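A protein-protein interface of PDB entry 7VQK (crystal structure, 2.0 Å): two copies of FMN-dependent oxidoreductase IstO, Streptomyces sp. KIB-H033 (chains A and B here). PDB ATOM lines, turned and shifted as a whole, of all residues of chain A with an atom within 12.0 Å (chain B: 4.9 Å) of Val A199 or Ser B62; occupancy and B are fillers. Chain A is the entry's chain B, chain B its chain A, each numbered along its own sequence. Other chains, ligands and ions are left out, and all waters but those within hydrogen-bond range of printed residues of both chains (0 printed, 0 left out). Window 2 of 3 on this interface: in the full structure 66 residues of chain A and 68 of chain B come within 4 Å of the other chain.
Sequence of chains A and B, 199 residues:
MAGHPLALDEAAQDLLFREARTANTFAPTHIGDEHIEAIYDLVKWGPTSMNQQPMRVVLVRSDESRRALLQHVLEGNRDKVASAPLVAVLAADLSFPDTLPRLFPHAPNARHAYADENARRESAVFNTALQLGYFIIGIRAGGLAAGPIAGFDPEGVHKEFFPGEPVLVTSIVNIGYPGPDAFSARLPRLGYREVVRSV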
ATOM      1  N   TYR A 192     -13.200   3.826  10.521  1.00  0.00           N
ATOM      2  CA  TYR A 192     -12.120   4.779  10.777  1.00  0.00           C
ATOM      3  C   TYR A 192     -10.980   4.128  11.555  1.00  0.00           C
ATOM      4  O   TYR A 192      -9.802   4.276  11.205  1.00  0.00           O
ATOM      5  CB  TYR A 192     -12.669   5.985  11.548  1.00  0.00           C
ATOM      6  CG  TYR A 192     -11.635   7.051  11.877  1.00  0.00           C
ATOM      7  CD1 TYR A 192     -11.313   8.036  10.951  1.00  0.00           C
ATOM      8  CD2 TYR A 192     -10.996   7.080  13.113  1.00  0.00           C
ATOM      9  CE1 TYR A 192     -10.375   9.025  11.246  1.00  0.00           C
ATOM     10  CE2 TYR A 192     -10.040   8.069  13.414  1.00  0.00           C
ATOM     11  CZ  TYR A 192      -9.745   9.028  12.475  1.00  0.00           C
ATOM     12  OH  TYR A 192      -8.817  10.008  12.739  1.00  0.00           O
ATOM     13  N   ARG A 193     -11.316   3.391  12.623  1.00  0.00           N
ATOM     14  CA  ARG A 193     -10.296   2.814  13.489  1.00  0.00           C
ATOM     15  C   ARG A 193      -9.496   1.732  12.787  1.00  0.00           C
ATOM     16  O   ARG A 193      -8.388   1.417  13.229  1.00  0.00           O
ATOM     17  CB  ARG A 193     -10.934   2.247  14.771  1.00  0.00           C
ATOM     18  CG  ARG A 193     -11.672   0.917  14.557  1.00  0.00           C
ATOM     19  CD  ARG A 193     -12.246   0.347  15.872  1.00  0.00           C
ATOM     20  NE  ARG A 193     -13.394   1.122  16.330  1.00  0.00           N
ATOM     21  CZ  ARG A 193     -14.608   1.055  15.802  1.00  0.00           C
ATOM     22  NH1 ARG A 193     -14.894   0.208  14.825  1.00  0.00           N
ATOM     23  NH2 ARG A 193     -15.560   1.867  16.257  1.00  0.00           N
ATOM     24  N   VAL A 195      -8.514   2.178   9.654  1.00  0.00           N
ATOM     25  CA  VAL A 195      -7.795   2.872   8.593  1.00  0.00           C
ATOM     26  C   VAL A 195      -6.768   3.854   9.147  1.00  0.00           C
ATOM     27  O   VAL A 195      -5.669   3.981   8.599  1.00  0.00           O
ATOM     28  CB  VAL A 195      -8.791   3.582   7.652  1.00  0.00           C
ATOM     29  CG1 VAL A 195      -8.061   4.527   6.681  1.00  0.00           C
ATOM     30  CG2 VAL A 195      -9.641   2.535   6.870  1.00  0.00           C
ATOM     31  N   VAL A 196      -7.096   4.531  10.250  1.00  0.00           N
ATOM     32  CA  VAL A 196      -6.319   5.646  10.780  1.00  0.00           C
ATOM     33  C   VAL A 196      -5.847   5.312  12.189  1.00  0.00           C
ATOM     34  O   VAL A 196      -6.592   4.730  12.984  1.00  0.00           O
ATOM     35  CB  VAL A 196      -7.155   6.946  10.791  1.00  0.00           C
ATOM     36  CG1 VAL A 196      -6.340   8.113  11.348  1.00  0.00           C
ATOM     37  CG2 VAL A 196      -7.717   7.251   9.390  1.00  0.00           C
ATOM     38  N   ARG A 197      -4.609   5.690  12.500  1.00  0.00           N
ATOM     39  CA  ARG A 197      -4.126   5.660  13.874  1.00  0.00           C
ATOM     40  C   ARG A 197      -3.245   6.885  14.088  1.00  0.00           C
ATOM     41  O   ARG A 197      -2.789   7.513  13.127  1.00  0.00           O
ATOM     42  CB  ARG A 197      -3.382   4.350  14.168  1.00  0.00           C
ATOM     43  CG  ARG A 197      -2.020   4.245  13.514  1.00  0.00           C
ATOM     44  CD  ARG A 197      -1.405   2.854  13.707  1.00  0.00           C
ATOM     45  NE  ARG A 197      -1.556   2.033  12.512  1.00  0.00           N
ATOM     46  CZ  ARG A 197      -0.549   1.604  11.762  1.00  0.00           C
ATOM     47  NH1 ARG A 197       0.710   1.889  12.066  1.00  0.00           N
ATOM     48  NH2 ARG A 197      -0.813   0.881  10.671  1.00  0.00           N
ATOM     49  N   SER A 198      -3.020   7.240  15.357  1.00  0.00           N
ATOM     50  CA  SER A 198      -2.281   8.448  15.698  1.00  0.00           C
ATOM     51  C   SER A 198      -1.013   8.104  16.466  1.00  0.00           C
ATOM     52  O   SER A 198      -0.950   7.097  17.175  1.00  0.00           O
ATOM     53  CB  SER A 198      -3.129   9.412  16.529  1.00  0.00           C
ATOM     54  OG  SER A 198      -4.368   9.667  15.903  1.00  0.00           O
ATOM     55  N   VAL A 199      -0.002   8.963  16.331  1.00  0.00           N
ATOM     56  CA  VAL A 199       1.249   8.787  17.054  1.00  0.00           C
ATOM     57  C   VAL A 199       1.838  10.147  17.461  1.00  0.00           C
ATOM     58  O   VAL A 199       1.288  11.194  17.105  1.00  0.00           O
ATOM     59  CB  VAL A 199       2.265   7.984  16.220  1.00  0.00           C
ATOM     60  CG1 VAL A 199       1.731   6.583  15.916  1.00  0.00           C
ATOM     61  CG2 VAL A 199       2.632   8.744  14.927  1.00  0.00           C
ATOM     62  N   VAL B  58      -1.402   7.009   9.075  1.00  0.00           N
ATOM     63  CA  VAL B  58      -0.849   7.299  10.393  1.00  0.00           C
ATOM     64  C   VAL B  58      -0.794   8.810  10.550  1.00  0.00           C
ATOM     65  O   VAL B  58      -0.173   9.503   9.730  1.00  0.00           O
ATOM     66  CB  VAL B  58       0.539   6.675  10.589  1.00  0.00           C
ATOM     67  CG1 VAL B  58       1.148   7.166  11.920  1.00  0.00           C
ATOM     68  CG2 VAL B  58       0.435   5.141  10.569  1.00  0.00           C
ATOM     69  N   LEU B  59      -1.446   9.320  11.595  1.00  0.00           N
ATOM     70  CA  LEU B  59      -1.447  10.745  11.901  1.00  0.00           C
ATOM     71  C   LEU B  59      -0.229  11.046  12.769  1.00  0.00           C
ATOM     72  O   LEU B  59      -0.163  10.629  13.930  1.00  0.00           O
ATOM     73  CB  LEU B  59      -2.745  11.155  12.592  1.00  0.00           C
ATOM     74  CG  LEU B  59      -4.033  10.966  11.767  1.00  0.00           C
ATOM     75  CD1 LEU B  59      -5.265  11.362  12.589  1.00  0.00           C
ATOM     76  CD2 LEU B  59      -3.987  11.754  10.445  1.00  0.00           C
ATOM     77  N   VAL B  60       0.736  11.754  12.193  1.00  0.00           N
ATOM     78  CA  VAL B  60       1.992  12.062  12.889  1.00  0.00           C
ATOM     79  C   VAL B  60       1.758  13.405  13.572  1.00  0.00           C
ATOM     80  O   VAL B  60       2.052  14.475  13.044  1.00  0.00           O
ATOM     81  CB  VAL B  60       3.187  12.077  11.929  1.00  0.00           C
ATOM     82  CG1 VAL B  60       4.493  12.367  12.672  1.00  0.00           C
ATOM     83  CG2 VAL B  60       3.272  10.742  11.192  1.00  0.00           C
ATOM     84  N   ARG B  61       1.165  13.344  14.762  1.00  0.00           N
ATOM     85  CA  ARG B  61       0.806  14.594  15.427  1.00  0.00           C
ATOM     86  C   ARG B  61       1.866  15.049  16.428  1.00  0.00           C
ATOM     87  O   ARG B  61       2.293  16.206  16.388  1.00  0.00           O
ATOM     88  CB  ARG B  61      -0.556  14.468  16.130  1.00  0.00           C
ATOM     89  CG  ARG B  61      -1.135  15.844  16.496  1.00  0.00           C
ATOM     90  CD  ARG B  61      -2.419  15.770  17.294  1.00  0.00           C
ATOM     91  NE  ARG B  61      -3.600  15.758  16.441  1.00  0.00           N
ATOM     92  CZ  ARG B  61      -4.269  14.655  16.141  1.00  0.00           C
ATOM     93  NH1 ARG B  61      -3.881  13.475  16.595  1.00  0.00           N
ATOM     94  NH2 ARG B  61      -5.340  14.734  15.355  1.00  0.00           N
ATOM     95  N   SER B  62       2.307  14.155  17.313  1.00  0.00           N
ATOM     96  CA  SER B  62       3.212  14.544  18.391  1.00  0.00           C
ATOM     97  C   SER B  62       4.551  15.038  17.844  1.00  0.00           C
ATOM     98  O   SER B  62       5.002  14.626  16.770  1.00  0.00           O
ATOM     99  CB  SER B  62       3.444  13.366  19.336  1.00  0.00           C
ATOM    100  OG  SER B  62       4.283  12.392  18.725  1.00  0.00           O
ATOM    101  N   ASP B  63       5.197  15.929  18.610  1.00  0.00           N
ATOM    102  CA  ASP B  63       6.532  16.393  18.230  1.00  0.00           C
ATOM    103  C   ASP B  63       7.492  15.220  18.119  1.00  0.00           C
ATOM    104  O   ASP B  63       8.330  15.177  17.215  1.00  0.00           O
ATOM    105  CB  ASP B  63       7.076  17.400  19.248  1.00  0.00           C
ATOM    106  CG  ASP B  63       6.404  18.757  19.166  1.00  0.00           C
ATOM    107  OD1 ASP B  63       5.680  19.015  18.182  1.00  0.00           O
ATOM    108  OD2 ASP B  63       6.595  19.565  20.107  1.00  0.00           O
ATOM    109  N   GLU B  64       7.386  14.265  19.045  1.00  0.00           N
ATOM    110  CA  GLU B  64       8.246  13.088  19.033  1.00  0.00           C
ATOM    111  C   GLU B  64       8.165  12.354  17.700  1.00  0.00           C
ATOM    112  O   GLU B  64       9.187  12.105  17.048  1.00  0.00           O
ATOM    113  CB  GLU B  64       7.858  12.159  20.188  1.00  0.00           C
ATOM    114  CG  GLU B  64       8.326  12.655  21.551  1.00  0.00           C
ATOM    115  CD  GLU B  64       7.399  13.686  22.158  1.00  0.00           C
ATOM    116  OE1 GLU B  64       6.296  13.883  21.614  1.00  0.00           O
ATOM    117  OE2 GLU B  64       7.772  14.296  23.188  1.00  0.00           O
ATOM    118  N   SER B  65       6.952  11.996  17.273  1.00  0.00           N
ATOM    119  CA  SER B  65       6.834  11.292  16.002  1.00  0.00           C
ATOM    120  C   SER B  65       7.211  12.195  14.836  1.00  0.00           C
ATOM    121  O   SER B  65       7.808  11.729  13.860  1.00  0.00           O
ATOM    122  CB  SER B  65       5.421  10.736  15.827  1.00  0.00           C
ATOM    123  OG  SER B  65       4.473  11.777  15.641  1.00  0.00           O
ATOM    124  N   ARG B  66       6.892  13.490  14.922  1.00  0.00           N
ATOM    125  CA  ARG B  66       7.242  14.390  13.833  1.00  0.00           C
ATOM    126  C   ARG B  66       8.754  14.456  13.640  1.00  0.00           C
ATOM    127  O   ARG B  66       9.243  14.452  12.508  1.00  0.00           O
ATOM    128  CB  ARG B  66       6.657  15.779  14.087  1.00  0.00           C
ATOM    129  CG  ARG B  66       6.524  16.623  12.828  1.00  0.00           C
ATOM    130  CD  ARG B  66       5.432  16.067  11.887  1.00  0.00           C
ATOM    131  NE  ARG B  66       4.095  16.334  12.411  1.00  0.00           N
ATOM    132  CZ  ARG B  66       3.580  17.543  12.586  1.00  0.00           C
ATOM    133  NH1 ARG B  66       4.221  18.633  12.187  1.00  0.00           N
ATOM    134  NH2 ARG B  66       2.404  17.666  13.199  1.00  0.00           N
ATOM    135  N   PHE B 161       6.994   3.990  11.083  1.00  0.00           N
ATOM    136  CA  PHE B 161       5.584   4.057  11.439  1.00  0.00           C
ATOM    137  C   PHE B 161       4.756   2.847  11.018  1.00  0.00           C
ATOM    138  O   PHE B 161       3.606   2.730  11.458  1.00  0.00           O
ATOM    139  CB  PHE B 161       4.941   5.320  10.842  1.00  0.00           C
ATOM    140  CG  PHE B 161       5.615   6.596  11.252  1.00  0.00           C
ATOM    141  CD1 PHE B 161       6.468   7.255  10.387  1.00  0.00           C
ATOM    142  CD2 PHE B 161       5.420   7.117  12.523  1.00  0.00           C
ATOM    143  CE1 PHE B 161       7.102   8.428  10.772  1.00  0.00           C
ATOM    144  CE2 PHE B 161       6.054   8.289  12.914  1.00  0.00           C
ATOM    145  CZ  PHE B 161       6.895   8.941  12.041  1.00  0.00           C
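Hydrophobic or aromatic side chains of chain A that line the printed part of chain B: Tyr A192, Val A196 and Val A199. Along chain A the printed residues that touch a printed residue of chain B span positions 192 to 199. Of the 10 printed residues of chain B, 7 touch a printed residue of chain A. Printed residues of chain B that touch a printed residue of chain A: Val B58, Leu B59, Val B60, Arg B61, Ser B62, Ser B65 and Phe B161. Hydrophobic or aromatic side chains of chain B within 4 Å of the printed part of chain A: Val B58, Leu B59 and Phe B161. Among the printed residues, 14 pairs touch across the chains. Among the printed residues, no Asp or Glu carboxylate lies within 4 Å of a Lys or Arg side-chain nitrogen of the other chain.
Of the printed residues of chain B, Tyr A192 touches Leu B59. Arg A193 touches none of the printed residues of chain B. Printed residues of chain B within 4 Å of Val A196: Leu B59 (3.6 Å). Of the printed residues of chain B, Arg A197 touches Val B58, Leu B59 and Phe B161. Of the printed residues of chain B, Ser A198 touches Leu B59 and Arg B61. Printed residues of chain B within 4 Å of Val A199: Val B58 (3.7 Å), Leu B59 (2.9 Å), Val B60 (3.9 Å), Arg B61 (3.2 Å), Ser B62 (3.1 Å), Ser B65 (3.5 Å) and Phe B161 (3.996 Å). Of chain A, only Arg A197 and Val A199 come within 4 Å of Val B58. Of chain A, only Val A199 comes within 4 Å of Val B60. Ser B62 touches one residue of chain A. No residue of chain A comes within 4 Å of Asp B63. Of chain A, only Val A199 comes within 4 Å of Ser B65. Arg B66 touches none of the printed residues of chain A. Of the printed residues of chain A, Phe B161 touches Arg A197 (3.1 Å) and Val A199 (3.996 Å). The nearest printed residue of chain B that does not touch Val A199 is Asp B63 (6.3 Å).
O of Val B60 sits at hydrogen-bond distance from NE of Arg B66, 2.8 Å away. The side-chain hydroxyl (OG) of Ser B62 sits at hydrogen-bond distance from the backbone NH (N) of Ser B65 (3.1 Å).
OH of Tyr A192 touches CD1 of Leu B59, 3.8 Å away. CG1 of Val A196 touches CD1 of Leu B59 (3.6 Å). Arg A197 touches Val B58. Ser A198 touches Leu B59 (CA to O, 3.5 Å). Arg B61 touches Ser A198. Val B58 touches Val A199. Val B60 touches Val A199 (CA to CG2, 3.9 Å). CB of Ser B65 touches CG2 of Val A199, 3.5 Å away. CE2 of Phe B161 touches CG2 of Val A199 (3.996 Å).
N of Leu B59 lies within hydrogen-bond range of O of Arg A197 (2.7 Å). The backbone carbonyl oxygen of Leu B59 is in hydrogen-bond range of the backbone NH of Val A199. The backbone carbonyl oxygen (O) of Val A199 sits at hydrogen-bond distance from the backbone NH (N) of Arg B61, 3.2 Å away. O of Val A199 lies within hydrogen-bond range of N of Ser B62 (3.1 Å). The backbone carbonyl oxygen (O) of Phe B161 sits at hydrogen-bond distance from the guanidinium group (NH1) of Arg A197.
No position is printed for both chains. Of the 14 pairs that touch across the chains among the printed residues, none has its exchanged pair printed and touching as well.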
